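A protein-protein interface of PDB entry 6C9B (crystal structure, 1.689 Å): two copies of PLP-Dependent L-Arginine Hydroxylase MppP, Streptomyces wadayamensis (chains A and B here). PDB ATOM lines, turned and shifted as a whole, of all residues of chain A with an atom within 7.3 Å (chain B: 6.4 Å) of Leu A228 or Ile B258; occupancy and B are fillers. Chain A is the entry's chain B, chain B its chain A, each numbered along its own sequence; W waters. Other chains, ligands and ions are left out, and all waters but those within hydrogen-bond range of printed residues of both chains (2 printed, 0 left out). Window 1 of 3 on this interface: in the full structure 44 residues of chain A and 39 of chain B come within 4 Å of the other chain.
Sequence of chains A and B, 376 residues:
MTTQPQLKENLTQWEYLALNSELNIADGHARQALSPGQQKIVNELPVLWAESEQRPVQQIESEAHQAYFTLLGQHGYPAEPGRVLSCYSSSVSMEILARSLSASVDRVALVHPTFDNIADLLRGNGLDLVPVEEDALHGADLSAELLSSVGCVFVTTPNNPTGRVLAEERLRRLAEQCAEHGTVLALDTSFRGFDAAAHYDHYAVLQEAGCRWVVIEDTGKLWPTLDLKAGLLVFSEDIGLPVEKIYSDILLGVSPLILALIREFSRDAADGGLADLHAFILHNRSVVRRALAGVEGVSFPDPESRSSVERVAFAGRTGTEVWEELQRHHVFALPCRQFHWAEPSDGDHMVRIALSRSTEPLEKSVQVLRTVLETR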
ATOM      1  N   LEU A  45       7.352 -27.876   7.687  1.00  0.00           N
ATOM      2  CA  LEU A  45       6.083 -28.246   8.305  1.00  0.00           C
ATOM      3  C   LEU A  45       5.173 -29.049   7.385  1.00  0.00           C
ATOM      4  O   LEU A  45       4.480 -29.945   7.889  1.00  0.00           O
ATOM      5  CB  LEU A  45       5.343 -26.996   8.794  1.00  0.00           C
ATOM      6  CG  LEU A  45       5.724 -26.539  10.189  1.00  0.00           C
ATOM      7  CD1 LEU A  45       5.184 -25.152  10.428  1.00  0.00           C
ATOM      8  CD2 LEU A  45       5.177 -27.518  11.212  1.00  0.00           C
ATOM      9  N   TYR A  88      -1.943 -31.168  26.518  1.00  0.00           N
ATOM     10  CA  TYR A  88      -1.884 -29.916  25.752  1.00  0.00           C
ATOM     11  C   TYR A  88      -0.932 -28.891  26.359  1.00  0.00           C
ATOM     12  O   TYR A  88      -0.368 -28.062  25.631  1.00  0.00           O
ATOM     13  CB  TYR A  88      -3.266 -29.281  25.644  1.00  0.00           C
ATOM     14  CG  TYR A  88      -4.325 -30.151  25.028  1.00  0.00           C
ATOM     15  CD1 TYR A  88      -4.192 -30.626  23.731  1.00  0.00           C
ATOM     16  CD2 TYR A  88      -5.471 -30.461  25.714  1.00  0.00           C
ATOM     17  CE1 TYR A  88      -5.185 -31.419  23.147  1.00  0.00           C
ATOM     18  CE2 TYR A  88      -6.470 -31.216  25.135  1.00  0.00           C
ATOM     19  CZ  TYR A  88      -6.312 -31.693  23.856  1.00  0.00           C
ATOM     20  OH  TYR A  88      -7.268 -32.463  23.276  1.00  0.00           O
ATOM     21  N   THR A 219       7.514 -28.491  27.416  1.00  0.00           N
ATOM     22  CA  THR A 219       8.377 -28.063  26.326  1.00  0.00           C
ATOM     23  C   THR A 219       8.164 -26.602  25.962  1.00  0.00           C
ATOM     24  O   THR A 219       8.958 -26.051  25.180  1.00  0.00           O
ATOM     25  CB  THR A 219       8.144 -28.903  25.061  1.00  0.00           C
ATOM     26  OG1 THR A 219       6.870 -28.565  24.502  1.00  0.00           O
ATOM     27  CG2 THR A 219       8.200 -30.356  25.342  1.00  0.00           C
ATOM     28  N   GLY A 220       7.128 -25.974  26.513  1.00  0.00           N
ATOM     29  CA  GLY A 220       6.619 -24.723  25.969  1.00  0.00           C
ATOM     30  C   GLY A 220       7.475 -23.497  26.192  1.00  0.00           C
ATOM     31  O   GLY A 220       7.395 -22.568  25.402  1.00  0.00           O
ATOM     32  N   TRP A 223      11.510 -22.786  23.579  1.00  0.00           N
ATOM     33  CA  TRP A 223      11.701 -22.425  22.188  1.00  0.00           C
ATOM     34  C   TRP A 223      10.519 -21.612  21.691  1.00  0.00           C
ATOM     35  O   TRP A 223       9.377 -21.827  22.132  1.00  0.00           O
ATOM     36  CB  TRP A 223      11.832 -23.674  21.315  1.00  0.00           C
ATOM     37  CG  TRP A 223      12.876 -24.613  21.724  1.00  0.00           C
ATOM     38  CD1 TRP A 223      14.204 -24.355  21.839  1.00  0.00           C
ATOM     39  CD2 TRP A 223      12.695 -25.990  22.080  1.00  0.00           C
ATOM     40  NE1 TRP A 223      14.873 -25.489  22.218  1.00  0.00           N
ATOM     41  CE2 TRP A 223      13.967 -26.511  22.362  1.00  0.00           C
ATOM     42  CE3 TRP A 223      11.582 -26.838  22.155  1.00  0.00           C
ATOM     43  CZ2 TRP A 223      14.170 -27.831  22.742  1.00  0.00           C
ATOM     44  CZ3 TRP A 223      11.788 -28.161  22.529  1.00  0.00           C
ATOM     45  CH2 TRP A 223      13.074 -28.642  22.814  1.00  0.00           C
ATOM     46  N   PRO A 224      10.747 -20.722  20.730  1.00  0.00           N
ATOM     47  CA  PRO A 224       9.666 -19.887  20.173  1.00  0.00           C
ATOM     48  C   PRO A 224       8.836 -20.636  19.138  1.00  0.00           C
ATOM     49  O   PRO A 224       8.935 -20.451  17.920  1.00  0.00           O
ATOM     50  CB  PRO A 224      10.425 -18.710  19.556  1.00  0.00           C
ATOM     51  CG  PRO A 224      11.737 -19.272  19.185  1.00  0.00           C
ATOM     52  CD  PRO A 224      12.068 -20.329  20.189  1.00  0.00           C
ATOM     53  N   THR A 225       7.936 -21.473  19.653  1.00  0.00           N
ATOM     54  CA  THR A 225       7.098 -22.337  18.838  1.00  0.00           C
ATOM     55  C   THR A 225       5.635 -21.890  18.805  1.00  0.00           C
ATOM     56  O   THR A 225       4.748 -22.700  18.505  1.00  0.00           O
ATOM     57  CB  THR A 225       7.162 -23.765  19.343  1.00  0.00           C
ATOM     58  OG1 THR A 225       6.697 -23.786  20.698  1.00  0.00           O
ATOM     59  CG2 THR A 225       8.581 -24.325  19.299  1.00  0.00           C
ATOM     60  N   LEU A 226       5.376 -20.605  19.035  1.00  0.00           N
ATOM     61  CA  LEU A 226       4.019 -20.050  18.934  1.00  0.00           C
ATOM     62  C   LEU A 226       3.085 -20.826  19.840  1.00  0.00           C
ATOM     63  O   LEU A 226       1.938 -21.093  19.488  1.00  0.00           O
ATOM     64  CB  LEU A 226       3.486 -20.068  17.497  1.00  0.00           C
ATOM     65  CG  LEU A 226       4.361 -19.351  16.461  1.00  0.00           C
ATOM     66  CD1 LEU A 226       3.802 -19.578  15.093  1.00  0.00           C
ATOM     67  CD2 LEU A 226       4.432 -17.872  16.772  1.00  0.00           C
ATOM     68  N   ASP A 227       3.594 -21.192  21.011  1.00  0.00           N
ATOM     69  CA  ASP A 227       2.809 -21.895  22.021  1.00  0.00           C
ATOM     70  C   ASP A 227       2.387 -23.293  21.580  1.00  0.00           C
ATOM     71  O   ASP A 227       1.433 -23.852  22.134  1.00  0.00           O
ATOM     72  CB  ASP A 227       1.560 -21.087  22.400  1.00  0.00           C
ATOM     73  CG  ASP A 227       1.847 -19.999  23.413  1.00  0.00           C
ATOM     74  OD1 ASP A 227       2.892 -19.320  23.291  1.00  0.00           O
ATOM     75  OD2 ASP A 227       1.005 -19.809  24.320  1.00  0.00           O
ATOM     76  N   LEU A 228       3.042 -23.861  20.568  1.00  0.00           N
ATOM     77  CA  LEU A 228       2.859 -25.253  20.198  1.00  0.00           C
ATOM     78  C   LEU A 228       3.782 -26.066  21.091  1.00  0.00           C
ATOM     79  O   LEU A 228       4.999 -25.891  21.055  1.00  0.00           O
ATOM     80  CB  LEU A 228       3.184 -25.462  18.724  1.00  0.00           C
ATOM     81  CG  LEU A 228       2.252 -24.666  17.801  1.00  0.00           C
ATOM     82  CD1 LEU A 228       2.853 -24.644  16.414  1.00  0.00           C
ATOM     83  CD2 LEU A 228       0.845 -25.232  17.760  1.00  0.00           C
ATOM     84  N   LYS A 229       3.209 -26.931  21.913  1.00  0.00           N
ATOM     85  CA  LYS A 229       3.943 -27.450  23.052  1.00  0.00           C
ATOM     86  C   LYS A 229       3.213 -28.663  23.607  1.00  0.00           C
ATOM     87  O   LYS A 229       2.094 -28.985  23.200  1.00  0.00           O
ATOM     88  CB  LYS A 229       4.055 -26.383  24.134  1.00  0.00           C
ATOM     89  CG  LYS A 229       2.686 -26.006  24.731  1.00  0.00           C
ATOM     90  CD  LYS A 229       2.628 -24.641  25.345  1.00  0.00           C
ATOM     91  CE  LYS A 229       1.179 -24.311  25.716  1.00  0.00           C
ATOM     92  NZ  LYS A 229       1.141 -23.023  26.454  1.00  0.00           N
ATOM     93  N   ALA A 230       3.848 -29.301  24.580  1.00  0.00           N
ATOM     94  CA  ALA A 230       3.163 -30.302  25.384  1.00  0.00           C
ATOM     95  C   ALA A 230       3.652 -30.213  26.811  1.00  0.00           C
ATOM     96  O   ALA A 230       4.833 -29.943  27.074  1.00  0.00           O
ATOM     97  CB  ALA A 230       3.375 -31.731  24.863  1.00  0.00           C
ATOM     98  N   SER A 255      -1.556 -33.555  19.342  1.00  0.00           N
ATOM     99  CA  SER A 255      -1.412 -33.653  17.900  1.00  0.00           C
ATOM    100  C   SER A 255      -0.085 -34.310  17.542  1.00  0.00           C
ATOM    101  O   SER A 255       0.964 -33.914  18.076  1.00  0.00           O
ATOM    102  CB  SER A 255      -1.470 -32.265  17.274  1.00  0.00           C
ATOM    103  OG  SER A 255      -1.046 -32.309  15.913  1.00  0.00           O
ATOM    104  N   LEU A 257       1.545 -33.647  14.957  1.00  0.00           N
ATOM    105  CA  LEU A 257       2.385 -32.595  14.394  1.00  0.00           C
ATOM    106  C   LEU A 257       3.151 -31.865  15.488  1.00  0.00           C
ATOM    107  O   LEU A 257       4.317 -31.497  15.298  1.00  0.00           O
ATOM    108  CB  LEU A 257       1.542 -31.602  13.596  1.00  0.00           C
ATOM    109  CG  LEU A 257       2.384 -30.555  12.846  1.00  0.00           C
ATOM    110  CD1 LEU A 257       3.080 -31.189  11.668  1.00  0.00           C
ATOM    111  CD2 LEU A 257       1.536 -29.394  12.355  1.00  0.00           C
ATOM    112  N   ILE A 258       2.509 -31.629  16.636  1.00  0.00           N
ATOM    113  CA  ILE A 258       3.202 -30.979  17.741  1.00  0.00           C
ATOM    114  C   ILE A 258       4.293 -31.883  18.291  1.00  0.00           C
ATOM    115  O   ILE A 258       5.399 -31.425  18.592  1.00  0.00           O
ATOM    116  CB  ILE A 258       2.188 -30.560  18.820  1.00  0.00           C
ATOM    117  CG1 ILE A 258       1.307 -29.457  18.280  1.00  0.00           C
ATOM    118  CG2 ILE A 258       2.892 -30.137  20.117  1.00  0.00           C
ATOM    119  CD1 ILE A 258       0.174 -29.067  19.206  1.00  0.00           C
ATOM    120  N   LEU A 261       7.102 -31.682  15.968  1.00  0.00           N
ATOM    121  CA  LEU A 261       7.824 -30.433  16.171  1.00  0.00           C
ATOM    122  C   LEU A 261       8.727 -30.508  17.395  1.00  0.00           C
ATOM    123  O   LEU A 261       9.869 -30.034  17.357  1.00  0.00           O
ATOM    124  CB  LEU A 261       6.840 -29.265  16.293  1.00  0.00           C
ATOM    125  CG  LEU A 261       6.266 -28.715  15.000  1.00  0.00           C
ATOM    126  CD1 LEU A 261       5.155 -27.733  15.304  1.00  0.00           C
ATOM    127  CD2 LEU A 261       7.380 -28.013  14.221  1.00  0.00           C
ATOM    128  N   ILE A 262       8.233 -31.086  18.492  1.00  0.00           N
ATOM    129  CA  ILE A 262       9.047 -31.207  19.694  1.00  0.00           C
ATOM    130  C   ILE A 262      10.276 -32.052  19.405  1.00  0.00           C
ATOM    131  O   ILE A 262      11.392 -31.756  19.862  1.00  0.00           O
ATOM    132  CB  ILE A 262       8.209 -31.817  20.823  1.00  0.00           C
ATOM    133  CG1 ILE A 262       7.159 -30.812  21.283  1.00  0.00           C
ATOM    134  CG2 ILE A 262       9.115 -32.259  21.983  1.00  0.00           C
ATOM    135  CD1 ILE A 262       6.103 -31.411  22.194  1.00  0.00           C
ATOM    136  N   TRP B  49       2.891 -19.403   9.821  1.00  0.00           N
ATOM    137  CA  TRP B  49       3.813 -19.231  10.944  1.00  0.00           C
ATOM    138  C   TRP B  49       4.346 -17.807  11.001  1.00  0.00           C
ATOM    139  O   TRP B  49       4.342 -17.166  12.053  1.00  0.00           O
ATOM    140  CB  TRP B  49       4.965 -20.238  10.830  1.00  0.00           C
ATOM    141  CG  TRP B  49       5.824 -20.287  12.054  1.00  0.00           C
ATOM    142  CD1 TRP B  49       6.643 -19.307  12.524  1.00  0.00           C
ATOM    143  CD2 TRP B  49       5.918 -21.372  12.985  1.00  0.00           C
ATOM    144  NE1 TRP B  49       7.242 -19.709  13.695  1.00  0.00           N
ATOM    145  CE2 TRP B  49       6.822 -20.976  13.994  1.00  0.00           C
ATOM    146  CE3 TRP B  49       5.340 -22.632  13.049  1.00  0.00           C
ATOM    147  CZ2 TRP B  49       7.157 -21.800  15.073  1.00  0.00           C
ATOM    148  CZ3 TRP B  49       5.666 -23.460  14.134  1.00  0.00           C
ATOM    149  CH2 TRP B  49       6.573 -23.037  15.117  1.00  0.00           C
ATOM    150  N   SER B  52       1.771 -15.476  12.263  1.00  0.00           N
ATOM    151  CA  SER B  52       1.527 -15.633  13.700  1.00  0.00           C
ATOM    152  C   SER B  52       2.641 -15.027  14.540  1.00  0.00           C
ATOM    153  O   SER B  52       2.402 -14.617  15.686  1.00  0.00           O
ATOM    154  CB  SER B  52       1.368 -17.116  14.031  1.00  0.00           C
ATOM    155  OG  SER B  52       0.298 -17.685  13.323  1.00  0.00           O
ATOM    156  N   ILE B  60      -5.731 -12.180  14.955  1.00  0.00           N
ATOM    157  CA  ILE B  60      -5.884 -13.498  14.357  1.00  0.00           C
ATOM    158  C   ILE B  60      -7.058 -14.215  15.001  1.00  0.00           C
ATOM    159  O   ILE B  60      -7.856 -14.875  14.325  1.00  0.00           O
ATOM    160  CB  ILE B  60      -4.581 -14.306  14.494  1.00  0.00           C
ATOM    161  CG1 ILE B  60      -3.410 -13.610  13.752  1.00  0.00           C
ATOM    162  CG2 ILE B  60      -4.790 -15.750  13.987  1.00  0.00           C
ATOM    163  CD1 ILE B  60      -2.058 -14.261  13.930  1.00  0.00           C
ATOM    164  N   ALA B  64     -10.426 -15.624  13.267  1.00  0.00           N
ATOM    165  CA  ALA B  64     -10.790 -17.033  13.312  1.00  0.00           C
ATOM    166  C   ALA B  64     -12.222 -17.206  13.812  1.00  0.00           C
ATOM    167  O   ALA B  64     -13.001 -17.984  13.250  1.00  0.00           O
ATOM    168  CB  ALA B  64      -9.802 -17.793  14.195  1.00  0.00           C
ATOM    169  N   THR B 219     -13.959 -26.780  17.034  1.00  0.00           N
ATOM    170  CA  THR B 219     -13.567 -26.918  15.636  1.00  0.00           C
ATOM    171  C   THR B 219     -13.059 -28.312  15.302  1.00  0.00           C
ATOM    172  O   THR B 219     -12.918 -28.644  14.113  1.00  0.00           O
ATOM    173  CB  THR B 219     -12.490 -25.883  15.261  1.00  0.00           C
ATOM    174  OG1 THR B 219     -11.242 -26.218  15.884  1.00  0.00           O
ATOM    175  CG2 THR B 219     -12.907 -24.482  15.705  1.00  0.00           C
ATOM    176  N   ASP B 227      -5.716 -33.058  14.802  1.00  0.00           N
ATOM    177  CA  ASP B 227      -6.141 -32.696  16.146  1.00  0.00           C
ATOM    178  C   ASP B 227      -5.664 -31.313  16.564  1.00  0.00           C
ATOM    179  O   ASP B 227      -5.574 -31.013  17.766  1.00  0.00           O
ATOM    180  CB  ASP B 227      -5.673 -33.742  17.162  1.00  0.00           C
ATOM    181  CG  ASP B 227      -6.645 -34.884  17.305  1.00  0.00           C
ATOM    182  OD1 ASP B 227      -6.975 -35.552  16.289  1.00  0.00           O
ATOM    183  OD2 ASP B 227      -7.073 -35.108  18.452  1.00  0.00           O
ATOM    184  N   LEU B 228      -5.337 -30.476  15.598  1.00  0.00           N
ATOM    185  CA  LEU B 228      -5.086 -29.059  15.815  1.00  0.00           C
ATOM    186  C   LEU B 228      -6.432 -28.350  15.773  1.00  0.00           C
ATOM    187  O   LEU B 228      -7.121 -28.342  14.738  1.00  0.00           O
ATOM    188  CB  LEU B 228      -4.140 -28.516  14.748  1.00  0.00           C
ATOM    189  CG  LEU B 228      -2.771 -29.192  14.750  1.00  0.00           C
ATOM    190  CD1 LEU B 228      -2.014 -28.840  13.480  1.00  0.00           C
ATOM    191  CD2 LEU B 228      -1.966 -28.764  15.972  1.00  0.00           C
ATOM    192  N   LYS B 229      -6.832 -27.785  16.898  1.00  0.00           N
ATOM    193  CA  LYS B 229      -8.216 -27.400  17.094  1.00  0.00           C
ATOM    194  C   LYS B 229      -8.309 -26.428  18.257  1.00  0.00           C
ATOM    195  O   LYS B 229      -7.337 -26.185  18.978  1.00  0.00           O
ATOM    196  CB  LYS B 229      -9.075 -28.639  17.407  1.00  0.00           C
ATOM    197  CG  LYS B 229      -8.566 -29.332  18.693  1.00  0.00           C
ATOM    198  CD  LYS B 229      -9.098 -30.733  18.872  1.00  0.00           C
ATOM    199  CE  LYS B 229      -8.463 -31.357  20.117  1.00  0.00           C
ATOM    200  NZ  LYS B 229      -8.892 -32.759  20.301  1.00  0.00           N
ATOM    201  N   ALA B 230      -9.521 -25.915  18.449  1.00  0.00           N
ATOM    202  CA  ALA B 230      -9.852 -25.194  19.662  1.00  0.00           C
ATOM    203  C   ALA B 230     -11.284 -25.479  20.074  1.00  0.00           C
ATOM    204  O   ALA B 230     -12.179 -25.676  19.250  1.00  0.00           O
ATOM    205  CB  ALA B 230      -9.665 -23.687  19.489  1.00  0.00           C
ATOM    206  N   VAL B 254      -4.665 -19.912  23.106  1.00  0.00           N
ATOM    207  CA  VAL B 254      -4.234 -20.977  22.217  1.00  0.00           C
ATOM    208  C   VAL B 254      -3.196 -20.437  21.248  1.00  0.00           C
ATOM    209  O   VAL B 254      -3.019 -19.229  21.104  1.00  0.00           O
ATOM    210  CB  VAL B 254      -5.393 -21.618  21.450  1.00  0.00           C
ATOM    211  CG1 VAL B 254      -6.345 -22.317  22.451  1.00  0.00           C
ATOM    212  CG2 VAL B 254      -6.099 -20.636  20.649  1.00  0.00           C
ATOM    213  N   SER B 255      -2.524 -21.351  20.554  1.00  0.00           N
ATOM    214  CA  SER B 255      -1.485 -20.947  19.594  1.00  0.00           C
ATOM    215  C   SER B 255      -2.072 -20.067  18.497  1.00  0.00           C
ATOM    216  O   SER B 255      -3.084 -20.441  17.880  1.00  0.00           O
ATOM    217  CB  SER B 255      -0.830 -22.160  18.946  1.00  0.00           C
ATOM    218  OG  SER B 255      -0.031 -21.756  17.831  1.00  0.00           O
ATOM    219  N   PRO B 256      -1.429 -18.939  18.159  1.00  0.00           N
ATOM    220  CA  PRO B 256      -1.906 -18.181  16.994  1.00  0.00           C
ATOM    221  C   PRO B 256      -1.877 -18.981  15.707  1.00  0.00           C
ATOM    222  O   PRO B 256      -2.660 -18.693  14.786  1.00  0.00           O
ATOM    223  CB  PRO B 256      -0.946 -16.980  16.925  1.00  0.00           C
ATOM    224  CG  PRO B 256       0.259 -17.377  17.700  1.00  0.00           C
ATOM    225  CD  PRO B 256      -0.299 -18.275  18.818  1.00  0.00           C
ATOM    226  N   LEU B 257      -0.973 -19.948  15.588  1.00  0.00           N
ATOM    227  CA  LEU B 257      -0.928 -20.754  14.381  1.00  0.00           C
ATOM    228  C   LEU B 257      -2.192 -21.580  14.247  1.00  0.00           C
ATOM    229  O   LEU B 257      -2.712 -21.749  13.148  1.00  0.00           O
ATOM    230  CB  LEU B 257       0.305 -21.653  14.387  1.00  0.00           C
ATOM    231  CG  LEU B 257       0.525 -22.438  13.102  1.00  0.00           C
ATOM    232  CD1 LEU B 257       0.930 -21.495  11.979  1.00  0.00           C
ATOM    233  CD2 LEU B 257       1.576 -23.505  13.251  1.00  0.00           C
ATOM    234  N   ILE B 258      -2.675 -22.147  15.355  1.00  0.00           N
ATOM    235  CA  ILE B 258      -3.900 -22.921  15.300  1.00  0.00           C
ATOM    236  C   ILE B 258      -5.083 -22.024  14.986  1.00  0.00           C
ATOM    237  O   ILE B 258      -5.982 -22.406  14.230  1.00  0.00           O
ATOM    238  CB  ILE B 258      -4.080 -23.680  16.628  1.00  0.00           C
ATOM    239  CG1 ILE B 258      -2.975 -24.717  16.727  1.00  0.00           C
ATOM    240  CG2 ILE B 258      -5.467 -24.320  16.685  1.00  0.00           C
ATOM    241  CD1 ILE B 258      -2.963 -25.530  18.043  1.00  0.00           C
ATOM    242  N   LEU B 259      -5.119 -20.829  15.571  1.00  0.00           N
ATOM    243  CA  LEU B 259      -6.183 -19.890  15.235  1.00  0.00           C
ATOM    244  C   LEU B 259      -6.134 -19.514  13.758  1.00  0.00           C
ATOM    245  O   LEU B 259      -7.174 -19.461  13.084  1.00  0.00           O
ATOM    246  CB  LEU B 259      -6.067 -18.639  16.110  1.00  0.00           C
ATOM    247  CG  LEU B 259      -6.381 -18.869  17.601  1.00  0.00           C
ATOM    248  CD1 LEU B 259      -5.938 -17.679  18.421  1.00  0.00           C
ATOM    249  CD2 LEU B 259      -7.880 -19.145  17.792  1.00  0.00           C
ATOM    250  N   ALA B 260      -4.941 -19.283  13.228  1.00  0.00           N
ATOM    251  CA  ALA B 260      -4.832 -18.985  11.798  1.00  0.00           C
ATOM    252  C   ALA B 260      -5.297 -20.168  10.963  1.00  0.00           C
ATOM    253  O   ALA B 260      -5.989 -19.995   9.953  1.00  0.00           O
ATOM    254  CB  ALA B 260      -3.398 -18.613  11.459  1.00  0.00           C
ATOM    255  N   LEU B 261      -4.943 -21.387  11.381  1.00  0.00           N
ATOM    256  CA  LEU B 261      -5.385 -22.573  10.661  1.00  0.00           C
ATOM    257  C   LEU B 261      -6.905 -22.688  10.672  1.00  0.00           C
ATOM    258  O   LEU B 261      -7.520 -23.008   9.652  1.00  0.00           O
ATOM    259  CB  LEU B 261      -4.736 -23.810  11.291  1.00  0.00           C
ATOM    260  CG  LEU B 261      -4.636 -25.111  10.515  1.00  0.00           C
ATOM    261  CD1 LEU B 261      -3.666 -24.926   9.369  1.00  0.00           C
ATOM    262  CD2 LEU B 261      -4.156 -26.224  11.438  1.00  0.00           C
ATOM    263  N   ILE B 262      -7.529 -22.456  11.833  1.00  0.00           N
ATOM    264  CA  ILE B 262      -8.985 -22.463  11.921  1.00  0.00           C
ATOM    265  C   ILE B 262      -9.581 -21.432  10.979  1.00  0.00           C
ATOM    266  O   ILE B 262     -10.577 -21.692  10.293  1.00  0.00           O
ATOM    267  CB  ILE B 262      -9.426 -22.204  13.368  1.00  0.00           C
ATOM    268  CG1 ILE B 262      -9.110 -23.431  14.199  1.00  0.00           C
ATOM    269  CG2 ILE B 262     -10.913 -21.853  13.448  1.00  0.00           C
ATOM    270  CD1 ILE B 262      -9.117 -23.156  15.693  1.00  0.00           C
ATOM    271  N   ARG B 263      -8.993 -20.240  10.949  1.00  0.00           N
ATOM    272  CA  ARG B 263      -9.470 -19.201  10.047  1.00  0.00           C
ATOM    273  C   ARG B 263      -9.438 -19.678   8.600  1.00  0.00           C
ATOM    274  O   ARG B 263     -10.429 -19.557   7.862  1.00  0.00           O
ATOM    275  CB  ARG B 263      -8.607 -17.949  10.227  1.00  0.00           C
ATOM    276  CG  ARG B 263      -9.081 -16.760   9.417  1.00  0.00           C
ATOM    277  CD  ARG B 263      -8.023 -15.680   9.384  1.00  0.00           C
ATOM    278  NE  ARG B 263      -6.834 -16.129   8.651  1.00  0.00           N
ATOM    279  CZ  ARG B 263      -5.596 -15.698   8.889  1.00  0.00           C
ATOM    280  NH1 ARG B 263      -5.365 -14.774   9.818  1.00  0.00           N
ATOM    281  NH2 ARG B 263      -4.587 -16.174   8.172  1.00  0.00           N
HETATM  282  O   HOH W   1      -6.942 -34.602  21.115  1.00  0.00           O
HETATM  283  O   HOH W   2       8.407 -18.399  16.139  1.00  0.00           O
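The side-chain amino group of Lys B229 lies within hydrogen-bond range of the side-chain hydroxyl of Tyr A88.
The side-chain hydroxyl of Ser B255 lies within hydrogen-bond range of the backbone carbonyl oxygen of Leu A226.
The side-chain hydroxyl of Ser B52 lies within hydrogen-bond range of the backbone carbonyl oxygen of Pro B256 (3.5 Å).
The side-chain hydroxyl (OG) of Ser B52 sits at hydrogen-bond distance from the backbone NH (N) of Leu B257, at 3.4 Å.
NZ of Lys B229 is in salt-bridge range of OD2 of Asp B227 (3.5 Å).
The backbone NH of Leu B257 lies within hydrogen-bond range of the side-chain hydroxyl of Ser B255 (3.0 Å).
OG1 of Thr A225 is in hydrogen-bond range of O of Leu A228 (2.7 Å).
OG of Ser A255 sits at hydrogen-bond distance from N of Leu A257, 3.1 Å away.
CE3 of Trp B49 touches CD1 of Leu A45, at 3.6 Å.
CZ2 of Trp B49 touches CA of Thr A225, at 3.8 Å.
Trp B49 touches Leu A226 (CD2 to CD1, 3.5 Å).
CB of Ser B52 touches CD1 of Leu A226, 3.6 Å away.
Ser B255 touches Leu A228 (OG to CD2, 3.6 Å).
Leu B257 touches Leu A228 (CD2 to CD1, 3.6 Å).
Leu A228 touches Ile B258 (CD2 to CD1, 3.8 Å).
Leu B228 touches Ser A255 (CD2 to OG, 3.7 Å).
Leu A257 touches Leu B228.
Ile A258 touches Leu B228.
Leu A228 touches just these residues of chain B: Trp B49 (3.8 Å), Ser B255 (3.6 Å), Leu B257 (3.6 Å) and Ile B258 (3.8 Å).
Of the printed residues of chain A, Ile B258 touches Leu A228 (3.8 Å).
Printed residues of chain A within 4 Å of Ser B52: Leu A226 (3.6 Å).
Of the printed residues of chain A, Lys B229 touches Tyr A88.
Lys A229 touches none of the printed residues of chain B.
Ala A230 touches none of the printed residues of chain B.
The nearest printed residue of chain A that does not touch Ser B255 is Asp A227 (4.1 Å).
Hydrophobic or aromatic side chains of chain A within 4 Å of the printed part of chain B: Leu A45, Tyr A88, Leu A226, Leu A228, Leu A257 and Ile A258.
Along chain A the printed residues that touch a printed residue of chain B span positions 45 to 258.
Printed residues of chain B that touch a printed residue of chain A: Trp B49, Ser B52, Leu B228, Lys B229, Ser B255, Pro B256, Leu B257 and Ile B258.
Along chain B the printed residues that touch a printed residue of chain A span positions 49 to 258.
Among the printed residues, no Asp or Glu carboxylate lies within 4 Å of a Lys or Arg side-chain nitrogen of the other chain.
Leu A228 touches Ser B255, and with the chains exchanged Ser A255 touches Leu B228.
Leu A228 touches Leu B257, and with the chains exchanged Leu A257 touches Leu B228.
Leu A228 touches Ile B258, and with the chains exchanged Ile A258 touches Leu B228.
Positions printed for both chains: 219, 227, 228, 229, 230, 255, 257, 258, 261 and 262.
Of the 15 pairs that touch across the chains among the printed residues, 6 have their exchanged pair printed and touching as well.
Water W1 lies within hydrogen-bond range of OD2 of Asp B227 (2.7 Å), NZ of Lys B229 (2.8 Å) and OH of Tyr A88 (3.1 Å).
Water W2 lies within hydrogen-bond range of the backbone carbonyl oxygen (O) of Pro A224 and the indole nitrogen (NE1) of Trp B49.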
